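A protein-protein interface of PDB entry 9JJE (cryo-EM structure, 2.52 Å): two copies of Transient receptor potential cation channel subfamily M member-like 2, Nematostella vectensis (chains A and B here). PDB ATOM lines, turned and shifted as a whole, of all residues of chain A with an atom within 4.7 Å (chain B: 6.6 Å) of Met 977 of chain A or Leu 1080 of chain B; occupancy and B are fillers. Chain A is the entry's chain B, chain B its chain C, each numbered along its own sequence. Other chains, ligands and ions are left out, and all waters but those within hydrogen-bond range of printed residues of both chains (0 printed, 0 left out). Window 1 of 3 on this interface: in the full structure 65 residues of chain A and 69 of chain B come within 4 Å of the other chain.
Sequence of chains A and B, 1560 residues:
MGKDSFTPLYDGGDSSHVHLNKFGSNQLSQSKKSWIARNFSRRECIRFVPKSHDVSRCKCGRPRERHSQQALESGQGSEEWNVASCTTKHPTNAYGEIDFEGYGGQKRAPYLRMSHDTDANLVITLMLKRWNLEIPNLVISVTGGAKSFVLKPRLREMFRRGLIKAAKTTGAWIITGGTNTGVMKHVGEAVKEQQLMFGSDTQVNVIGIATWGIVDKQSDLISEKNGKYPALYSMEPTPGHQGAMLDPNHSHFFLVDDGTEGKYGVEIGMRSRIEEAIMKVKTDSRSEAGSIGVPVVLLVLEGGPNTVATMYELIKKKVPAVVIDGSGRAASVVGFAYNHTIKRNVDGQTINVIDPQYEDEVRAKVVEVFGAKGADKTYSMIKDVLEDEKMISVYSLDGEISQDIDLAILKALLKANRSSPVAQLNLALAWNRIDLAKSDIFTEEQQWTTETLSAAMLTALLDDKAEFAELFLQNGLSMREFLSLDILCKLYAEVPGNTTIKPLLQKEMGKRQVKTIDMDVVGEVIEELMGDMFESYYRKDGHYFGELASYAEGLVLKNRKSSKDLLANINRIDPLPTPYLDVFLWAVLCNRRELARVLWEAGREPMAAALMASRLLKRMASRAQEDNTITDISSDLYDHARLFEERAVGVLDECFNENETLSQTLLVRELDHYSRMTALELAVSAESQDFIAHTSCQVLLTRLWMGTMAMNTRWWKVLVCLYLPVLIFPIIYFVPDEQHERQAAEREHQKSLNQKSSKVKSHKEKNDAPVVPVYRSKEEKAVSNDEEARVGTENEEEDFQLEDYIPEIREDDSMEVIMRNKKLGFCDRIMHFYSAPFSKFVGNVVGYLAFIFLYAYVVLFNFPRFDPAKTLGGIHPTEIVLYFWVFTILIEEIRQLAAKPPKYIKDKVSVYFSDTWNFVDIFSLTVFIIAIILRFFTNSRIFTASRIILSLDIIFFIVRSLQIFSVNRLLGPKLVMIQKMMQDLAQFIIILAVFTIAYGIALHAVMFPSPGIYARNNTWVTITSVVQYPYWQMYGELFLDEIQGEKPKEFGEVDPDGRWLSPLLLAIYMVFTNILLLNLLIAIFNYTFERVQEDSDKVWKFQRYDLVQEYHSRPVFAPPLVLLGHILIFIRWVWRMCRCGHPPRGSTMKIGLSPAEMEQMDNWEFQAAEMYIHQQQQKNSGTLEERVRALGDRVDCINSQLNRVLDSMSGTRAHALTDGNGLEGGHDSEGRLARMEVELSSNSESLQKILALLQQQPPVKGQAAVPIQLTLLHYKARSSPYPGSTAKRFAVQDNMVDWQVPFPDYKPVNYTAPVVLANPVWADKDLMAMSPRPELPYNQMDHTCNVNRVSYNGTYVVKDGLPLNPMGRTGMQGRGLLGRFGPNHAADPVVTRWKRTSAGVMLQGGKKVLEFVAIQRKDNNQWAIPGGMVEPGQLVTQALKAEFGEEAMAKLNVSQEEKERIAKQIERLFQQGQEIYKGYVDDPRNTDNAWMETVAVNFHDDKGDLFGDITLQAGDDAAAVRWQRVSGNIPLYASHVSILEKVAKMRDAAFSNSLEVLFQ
CB of Lys 974 of chain A touches CD1 of Ile 991 of chain B, at 3.8 Å. Lys 974 of chain A touches Ile 1084 of chain B (CE to CD1, 3.7 Å). Ile 991 of chain B touches Leu 975 of chain A. CD1 of Leu 1080 of chain B touches SD of Met 977 of chain A, at 3.8 Å. CG2 of Ile 991 of chain B touches CD1 of Ile 978 of chain A (3.8 Å). Met 981 of chain A touches Leu 1076 of chain B. Leu 1080 of chain B touches Met 981 of chain A. Leu 1080 of chain B touches Phe 1089 of chain A. CE2 of Phe 1089 of chain A touches O of Ala 1083 of chain B, at 3.2 Å. Phe 1089 of chain A touches Ile 1084 of chain B.
Of the printed residues of chain B, Lys 974 of chain A touches Ile 991 and Ile 1084. Of the printed residues of chain B, Leu 975 of chain A touches Ile 991 (3.7 Å). Lys 980 of chain A touches none of the printed residues of chain B. Of the printed residues of chain A, Leu 1077 of chain B touches Ile 978 (3.8 Å). Leu 1080 of chain B touches four residues of chain A. Of the printed residues of chain A, Ile 1084 of chain B touches Lys 974 (3.7 Å) and Phe 1089 (3.6 Å). The nearest residue of chain B that does not touch Met 977 of chain A is Leu 1076 of chain B (5.4 Å). The nearest residue of chain A that does not touch Leu 1080 of chain B is Lys 974 of chain A (4.1 Å). The nearest printed residue of chain A that does not touch Leu 1077 of chain B is Met 981 of chain A (6.0 Å).
Of the 13 printed residues of chain B, 6 touch a printed residue of chain A. Among the printed residues, no Asp or Glu carboxylate lies within 4 Å of a Lys or Arg side-chain nitrogen of the other chain.
No position is printed for both chains. Of the 12 pairs that touch across the chains among the printed residues, none has its exchanged pair printed and touching as well.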
ATOM      1  N   PRO A 973       9.170 -16.446 -16.323  1.00  0.00           N
ATOM      2  CA  PRO A 973      10.151 -17.474 -15.938  1.00  0.00           C
ATOM      3  C   PRO A 973      11.191 -16.996 -14.941  1.00  0.00           C
ATOM      4  O   PRO A 973      11.604 -17.790 -14.089  1.00  0.00           O
ATOM      5  CB  PRO A 973      10.786 -17.865 -17.277  1.00  0.00           C
ATOM      6  CG  PRO A 973       9.709 -17.667 -18.242  1.00  0.00           C
ATOM      7  CD  PRO A 973       8.935 -16.471 -17.781  1.00  0.00           C
ATOM      8  N   LYS A 974      11.594 -15.719 -14.984  1.00  0.00           N
ATOM      9  CA  LYS A 974      12.488 -15.210 -13.947  1.00  0.00           C
ATOM     10  C   LYS A 974      11.785 -15.135 -12.599  1.00  0.00           C
ATOM     11  O   LYS A 974      12.425 -15.334 -11.566  1.00  0.00           O
ATOM     12  CB  LYS A 974      13.041 -13.833 -14.319  1.00  0.00           C
ATOM     13  CG  LYS A 974      13.666 -13.772 -15.693  1.00  0.00           C
ATOM     14  CD  LYS A 974      14.832 -14.722 -15.856  1.00  0.00           C
ATOM     15  CE  LYS A 974      15.452 -14.576 -17.228  1.00  0.00           C
ATOM     16  NZ  LYS A 974      14.561 -15.071 -18.305  1.00  0.00           N
ATOM     17  N   LEU A 975      10.471 -14.884 -12.590  1.00  0.00           N
ATOM     18  CA  LEU A 975       9.726 -14.934 -11.330  1.00  0.00           C
ATOM     19  C   LEU A 975       9.610 -16.358 -10.787  1.00  0.00           C
ATOM     20  O   LEU A 975       9.660 -16.561  -9.566  1.00  0.00           O
ATOM     21  CB  LEU A 975       8.335 -14.321 -11.503  1.00  0.00           C
ATOM     22  CG  LEU A 975       8.178 -12.826 -11.197  1.00  0.00           C
ATOM     23  CD1 LEU A 975       8.549 -12.572  -9.746  1.00  0.00           C
ATOM     24  CD2 LEU A 975       8.976 -11.922 -12.123  1.00  0.00           C
ATOM     25  N   VAL A 976       9.457 -17.346 -11.674  1.00  0.00           N
ATOM     26  CA  VAL A 976       9.480 -18.751 -11.255  1.00  0.00           C
ATOM     27  C   VAL A 976      10.855 -19.118 -10.694  1.00  0.00           C
ATOM     28  O   VAL A 976      10.969 -19.858  -9.701  1.00  0.00           O
ATOM     29  CB  VAL A 976       9.066 -19.658 -12.433  1.00  0.00           C
ATOM     30  CG1 VAL A 976       9.176 -21.135 -12.076  1.00  0.00           C
ATOM     31  CG2 VAL A 976       7.646 -19.337 -12.859  1.00  0.00           C
ATOM     32  N   MET A 977      11.915 -18.570 -11.300  1.00  0.00           N
ATOM     33  CA  MET A 977      13.270 -18.718 -10.772  1.00  0.00           C
ATOM     34  C   MET A 977      13.402 -18.108  -9.384  1.00  0.00           C
ATOM     35  O   MET A 977      14.013 -18.705  -8.498  1.00  0.00           O
ATOM     36  CB  MET A 977      14.275 -18.079 -11.728  1.00  0.00           C
ATOM     37  CG  MET A 977      14.440 -18.846 -13.005  1.00  0.00           C
ATOM     38  SD  MET A 977      15.334 -17.947 -14.271  1.00  0.00           S
ATOM     39  CE  MET A 977      15.144 -19.067 -15.656  1.00  0.00           C
ATOM     40  N   ILE A 978      12.832 -16.913  -9.183  1.00  0.00           N
ATOM     41  CA  ILE A 978      12.860 -16.251  -7.876  1.00  0.00           C
ATOM     42  C   ILE A 978      12.135 -17.087  -6.825  1.00  0.00           C
ATOM     43  O   ILE A 978      12.617 -17.244  -5.697  1.00  0.00           O
ATOM     44  CB  ILE A 978      12.270 -14.829  -7.989  1.00  0.00           C
ATOM     45  CG1 ILE A 978      13.212 -13.919  -8.775  1.00  0.00           C
ATOM     46  CG2 ILE A 978      12.000 -14.214  -6.627  1.00  0.00           C
ATOM     47  CD1 ILE A 978      12.575 -12.618  -9.196  1.00  0.00           C
ATOM     48  N   GLN A 979      11.005 -17.691  -7.203  1.00  0.00           N
ATOM     49  CA  GLN A 979      10.235 -18.511  -6.268  1.00  0.00           C
ATOM     50  C   GLN A 979      10.991 -19.783  -5.872  1.00  0.00           C
ATOM     51  O   GLN A 979      11.077 -20.125  -4.680  1.00  0.00           O
ATOM     52  CB  GLN A 979       8.876 -18.835  -6.893  1.00  0.00           C
ATOM     53  CG  GLN A 979       7.840 -19.445  -5.965  1.00  0.00           C
ATOM     54  CD  GLN A 979       7.865 -20.958  -5.967  1.00  0.00           C
ATOM     55  OE1 GLN A 979       8.257 -21.583  -6.952  1.00  0.00           O
ATOM     56  NE2 GLN A 979       7.426 -21.556  -4.868  1.00  0.00           N
ATOM     57  N   LYS A 980      11.589 -20.473  -6.849  1.00  0.00           N
ATOM     58  CA  LYS A 980      12.327 -21.691  -6.521  1.00  0.00           C
ATOM     59  C   LYS A 980      13.649 -21.388  -5.814  1.00  0.00           C
ATOM     60  O   LYS A 980      14.093 -22.174  -4.968  1.00  0.00           O
ATOM     61  CB  LYS A 980      12.554 -22.520  -7.783  1.00  0.00           C
ATOM     62  CG  LYS A 980      11.276 -23.084  -8.383  1.00  0.00           C
ATOM     63  CD  LYS A 980      11.564 -23.957  -9.591  1.00  0.00           C
ATOM     64  CE  LYS A 980      10.275 -24.427 -10.245  1.00  0.00           C
ATOM     65  NZ  LYS A 980       9.512 -25.353  -9.364  1.00  0.00           N
ATOM     66  N   MET A 981      14.267 -20.237  -6.101  1.00  0.00           N
ATOM     67  CA  MET A 981      15.455 -19.835  -5.355  1.00  0.00           C
ATOM     68  C   MET A 981      15.115 -19.402  -3.937  1.00  0.00           C
ATOM     69  O   MET A 981      15.945 -19.550  -3.040  1.00  0.00           O
ATOM     70  CB  MET A 981      16.195 -18.709  -6.074  1.00  0.00           C
ATOM     71  CG  MET A 981      16.946 -19.116  -7.325  1.00  0.00           C
ATOM     72  SD  MET A 981      17.616 -17.664  -8.151  1.00  0.00           S
ATOM     73  CE  MET A 981      18.152 -18.400  -9.685  1.00  0.00           C
ATOM     74  N   THR A1088      19.363 -24.241  -9.909  1.00  0.00           N
ATOM     75  CA  THR A1088      17.949 -23.908 -10.069  1.00  0.00           C
ATOM     76  C   THR A1088      17.706 -23.103 -11.345  1.00  0.00           C
ATOM     77  O   THR A1088      16.731 -23.345 -12.072  1.00  0.00           O
ATOM     78  CB  THR A1088      17.477 -23.133  -8.837  1.00  0.00           C
ATOM     79  OG1 THR A1088      17.656 -23.943  -7.669  1.00  0.00           O
ATOM     80  CG2 THR A1088      16.020 -22.744  -8.954  1.00  0.00           C
ATOM     81  N   PHE A1089      18.600 -22.145 -11.629  1.00  0.00           N
ATOM     82  CA  PHE A1089      18.530 -21.345 -12.849  1.00  0.00           C
ATOM     83  C   PHE A1089      18.600 -22.211 -14.094  1.00  0.00           C
ATOM     84  O   PHE A1089      17.858 -21.979 -15.050  1.00  0.00           O
ATOM     85  CB  PHE A1089      19.662 -20.316 -12.894  1.00  0.00           C
ATOM     86  CG  PHE A1089      19.662 -19.482 -14.151  1.00  0.00           C
ATOM     87  CD1 PHE A1089      18.773 -18.433 -14.291  1.00  0.00           C
ATOM     88  CD2 PHE A1089      20.536 -19.760 -15.205  1.00  0.00           C
ATOM     89  CE1 PHE A1089      18.746 -17.671 -15.442  1.00  0.00           C
ATOM     90  CE2 PHE A1089      20.513 -19.005 -16.358  1.00  0.00           C
ATOM     91  CZ  PHE A1089      19.620 -17.956 -16.477  1.00  0.00           C
ATOM     92  N   VAL A1092      15.372 -24.270 -14.528  1.00  0.00           N
ATOM     93  CA  VAL A1092      14.213 -23.522 -15.007  1.00  0.00           C
ATOM     94  C   VAL A1092      14.464 -22.975 -16.414  1.00  0.00           C
ATOM     95  O   VAL A1092      13.557 -22.970 -17.249  1.00  0.00           O
ATOM     96  CB  VAL A1092      13.829 -22.417 -14.004  1.00  0.00           C
ATOM     97  CG1 VAL A1092      12.610 -21.633 -14.489  1.00  0.00           C
ATOM     98  CG2 VAL A1092      13.521 -23.028 -12.653  1.00  0.00           C
ATOM     99  N   GLN A1093      15.699 -22.561 -16.715  1.00  0.00           N
ATOM    100  CA  GLN A1093      16.023 -21.949 -18.001  1.00  0.00           C
ATOM    101  C   GLN A1093      15.955 -22.953 -19.145  1.00  0.00           C
ATOM    102  O   GLN A1093      15.642 -22.573 -20.280  1.00  0.00           O
ATOM    103  CB  GLN A1093      17.414 -21.306 -17.917  1.00  0.00           C
ATOM    104  CG  GLN A1093      17.886 -20.552 -19.158  1.00  0.00           C
ATOM    105  CD  GLN A1093      17.066 -19.309 -19.445  1.00  0.00           C
ATOM    106  OE1 GLN A1093      16.724 -18.553 -18.537  1.00  0.00           O
ATOM    107  NE2 GLN A1093      16.749 -19.092 -20.716  1.00  0.00           N
ATOM    108  N   PHE B 988      15.910  -7.518 -17.213  1.00  0.00           N
ATOM    109  CA  PHE B 988      15.869  -7.809 -15.778  1.00  0.00           C
ATOM    110  C   PHE B 988      15.703  -6.557 -14.911  1.00  0.00           C
ATOM    111  O   PHE B 988      15.321  -6.671 -13.730  1.00  0.00           O
ATOM    112  CB  PHE B 988      17.146  -8.575 -15.391  1.00  0.00           C
ATOM    113  CG  PHE B 988      17.196  -9.019 -13.952  1.00  0.00           C
ATOM    114  CD1 PHE B 988      16.451 -10.107 -13.517  1.00  0.00           C
ATOM    115  CD2 PHE B 988      17.986  -8.342 -13.033  1.00  0.00           C
ATOM    116  CE1 PHE B 988      16.499 -10.511 -12.193  1.00  0.00           C
ATOM    117  CE2 PHE B 988      18.037  -8.739 -11.709  1.00  0.00           C
ATOM    118  CZ  PHE B 988      17.293  -9.826 -11.289  1.00  0.00           C
ATOM    119  N   ILE B 991      12.399  -6.014 -12.881  1.00  0.00           N
ATOM    120  CA  ILE B 991      12.265  -6.828 -11.674  1.00  0.00           C
ATOM    121  C   ILE B 991      13.150  -6.272 -10.564  1.00  0.00           C
ATOM    122  O   ILE B 991      12.728  -6.149  -9.397  1.00  0.00           O
ATOM    123  CB  ILE B 991      12.610  -8.296 -11.992  1.00  0.00           C
ATOM    124  CG1 ILE B 991      11.613  -8.890 -12.986  1.00  0.00           C
ATOM    125  CG2 ILE B 991      12.661  -9.142 -10.737  1.00  0.00           C
ATOM    126  CD1 ILE B 991      12.026 -10.253 -13.494  1.00  0.00           C
ATOM    127  N   ILE B1075      22.217 -11.502  -2.886  1.00  0.00           N
ATOM    128  CA  ILE B1075      22.484 -12.933  -3.022  1.00  0.00           C
ATOM    129  C   ILE B1075      21.606 -13.570  -4.093  1.00  0.00           C
ATOM    130  O   ILE B1075      22.092 -14.318  -4.942  1.00  0.00           O
ATOM    131  CB  ILE B1075      22.320 -13.651  -1.662  1.00  0.00           C
ATOM    132  CG1 ILE B1075      23.353 -13.156  -0.653  1.00  0.00           C
ATOM    133  CG2 ILE B1075      22.486 -15.150  -1.816  1.00  0.00           C
ATOM    134  CD1 ILE B1075      23.175 -13.766   0.727  1.00  0.00           C
ATOM    135  N   LEU B1076      20.300 -13.308  -4.084  1.00  0.00           N
ATOM    136  CA  LEU B1076      19.412 -14.047  -4.975  1.00  0.00           C
ATOM    137  C   LEU B1076      19.211 -13.340  -6.317  1.00  0.00           C
ATOM    138  O   LEU B1076      19.421 -13.946  -7.372  1.00  0.00           O
ATOM    139  CB  LEU B1076      18.073 -14.300  -4.267  1.00  0.00           C
ATOM    140  CG  LEU B1076      17.001 -15.259  -4.794  1.00  0.00           C
ATOM    141  CD1 LEU B1076      16.273 -15.873  -3.609  1.00  0.00           C
ATOM    142  CD2 LEU B1076      15.997 -14.577  -5.716  1.00  0.00           C
ATOM    143  N   LEU B1077      18.837 -12.056  -6.292  1.00  0.00           N
ATOM    144  CA  LEU B1077      18.519 -11.331  -7.523  1.00  0.00           C
ATOM    145  C   LEU B1077      19.760 -11.045  -8.363  1.00  0.00           C
ATOM    146  O   LEU B1077      19.742 -11.229  -9.588  1.00  0.00           O
ATOM    147  CB  LEU B1077      17.813 -10.015  -7.190  1.00  0.00           C
ATOM    148  CG  LEU B1077      16.403 -10.068  -6.601  1.00  0.00           C
ATOM    149  CD1 LEU B1077      15.951  -8.678  -6.184  1.00  0.00           C
ATOM    150  CD2 LEU B1077      15.436 -10.667  -7.603  1.00  0.00           C
ATOM    151  N   LEU B1078      20.843 -10.604  -7.722  1.00  0.00           N
ATOM    152  CA  LEU B1078      22.058 -10.276  -8.462  1.00  0.00           C
ATOM    153  C   LEU B1078      22.728 -11.513  -9.032  1.00  0.00           C
ATOM    154  O   LEU B1078      23.210 -11.487 -10.165  1.00  0.00           O
ATOM    155  CB  LEU B1078      23.027  -9.485  -7.585  1.00  0.00           C
ATOM    156  CG  LEU B1078      22.994  -7.984  -7.878  1.00  0.00           C
ATOM    157  CD1 LEU B1078      21.633  -7.403  -7.610  1.00  0.00           C
ATOM    158  CD2 LEU B1078      24.050  -7.257  -7.059  1.00  0.00           C
ATOM    159  N   ASN B1079      22.734 -12.616  -8.292  1.00  0.00           N
ATOM    160  CA  ASN B1079      23.304 -13.839  -8.836  1.00  0.00           C
ATOM    161  C   ASN B1079      22.373 -14.509  -9.834  1.00  0.00           C
ATOM    162  O   ASN B1079      22.852 -15.241 -10.704  1.00  0.00           O
ATOM    163  CB  ASN B1079      23.663 -14.782  -7.695  1.00  0.00           C
ATOM    164  CG  ASN B1079      24.772 -14.227  -6.827  1.00  0.00           C
ATOM    165  OD1 ASN B1079      25.826 -13.837  -7.326  1.00  0.00           O
ATOM    166  ND2 ASN B1079      24.505 -14.106  -5.532  1.00  0.00           N
ATOM    167  N   LEU B1080      21.066 -14.230  -9.764  1.00  0.00           N
ATOM    168  CA  LEU B1080      20.169 -14.566 -10.868  1.00  0.00           C
ATOM    169  C   LEU B1080      20.548 -13.811 -12.136  1.00  0.00           C
ATOM    170  O   LEU B1080      20.581 -14.396 -13.225  1.00  0.00           O
ATOM    171  CB  LEU B1080      18.721 -14.267 -10.476  1.00  0.00           C
ATOM    172  CG  LEU B1080      17.622 -14.365 -11.540  1.00  0.00           C
ATOM    173  CD1 LEU B1080      17.528 -15.750 -12.149  1.00  0.00           C
ATOM    174  CD2 LEU B1080      16.278 -13.957 -10.948  1.00  0.00           C
ATOM    175  N   LEU B1081      20.847 -12.517 -12.007  1.00  0.00           N
ATOM    176  CA  LEU B1081      21.274 -11.725 -13.160  1.00  0.00           C
ATOM    177  C   LEU B1081      22.636 -12.183 -13.687  1.00  0.00           C
ATOM    178  O   LEU B1081      22.866 -12.209 -14.904  1.00  0.00           O
ATOM    179  CB  LEU B1081      21.297 -10.247 -12.777  1.00  0.00           C
ATOM    180  CG  LEU B1081      21.703  -9.238 -13.846  1.00  0.00           C
ATOM    181  CD1 LEU B1081      20.803  -9.367 -15.058  1.00  0.00           C
ATOM    182  CD2 LEU B1081      21.609  -7.845 -13.262  1.00  0.00           C
ATOM    183  N   ILE B1082      23.541 -12.567 -12.780  1.00  0.00           N
ATOM    184  CA  ILE B1082      24.828 -13.144 -13.167  1.00  0.00           C
ATOM    185  C   ILE B1082      24.624 -14.478 -13.878  1.00  0.00           C
ATOM    186  O   ILE B1082      25.333 -14.800 -14.836  1.00  0.00           O
ATOM    187  CB  ILE B1082      25.740 -13.278 -11.927  1.00  0.00           C
ATOM    188  CG1 ILE B1082      26.116 -11.902 -11.385  1.00  0.00           C
ATOM    189  CG2 ILE B1082      27.028 -14.028 -12.234  1.00  0.00           C
ATOM    190  CD1 ILE B1082      26.758 -11.939 -10.014  1.00  0.00           C
ATOM    191  N   ALA B1083      23.621 -15.253 -13.455  1.00  0.00           N
ATOM    192  CA  ALA B1083      23.317 -16.517 -14.116  1.00  0.00           C
ATOM    193  C   ALA B1083      22.750 -16.299 -15.516  1.00  0.00           C
ATOM    194  O   ALA B1083      23.056 -17.066 -16.438  1.00  0.00           O
ATOM    195  CB  ALA B1083      22.342 -17.321 -13.260  1.00  0.00           C
ATOM    196  N   ILE B1084      21.922 -15.260 -15.685  1.00  0.00           N
ATOM    197  CA  ILE B1084      21.448 -14.865 -17.015  1.00  0.00           C
ATOM    198  C   ILE B1084      22.623 -14.466 -17.901  1.00  0.00           C
ATOM    199  O   ILE B1084      22.706 -14.861 -19.076  1.00  0.00           O
ATOM    200  CB  ILE B1084      20.425 -13.719 -16.898  1.00  0.00           C
ATOM    201  CG1 ILE B1084      19.194 -14.157 -16.115  1.00  0.00           C
ATOM    202  CG2 ILE B1084      19.978 -13.251 -18.267  1.00  0.00           C
ATOM    203  CD1 ILE B1084      18.377 -12.994 -15.602  1.00  0.00           C
ATOM    204  N   PHE B1085      23.561 -13.699 -17.335  1.00  0.00           N
ATOM    205  CA  PHE B1085      24.751 -13.288 -18.075  1.00  0.00           C
ATOM    206  C   PHE B1085      25.623 -14.483 -18.438  1.00  0.00           C
ATOM    207  O   PHE B1085      26.197 -14.528 -19.526  1.00  0.00           O
ATOM    208  CB  PHE B1085      25.561 -12.276 -17.261  1.00  0.00           C
ATOM    209  CG  PHE B1085      24.919 -10.917 -17.142  1.00  0.00           C
ATOM    210  CD1 PHE B1085      23.849 -10.547 -17.949  1.00  0.00           C
ATOM    211  CD2 PHE B1085      25.407 -10.000 -16.224  1.00  0.00           C
ATOM    212  CE1 PHE B1085      23.274  -9.294 -17.827  1.00  0.00           C
ATOM    213  CE2 PHE B1085      24.840  -8.746 -16.104  1.00  0.00           C
ATOM    214  CZ  PHE B1085      23.773  -8.393 -16.907  1.00  0.00           C
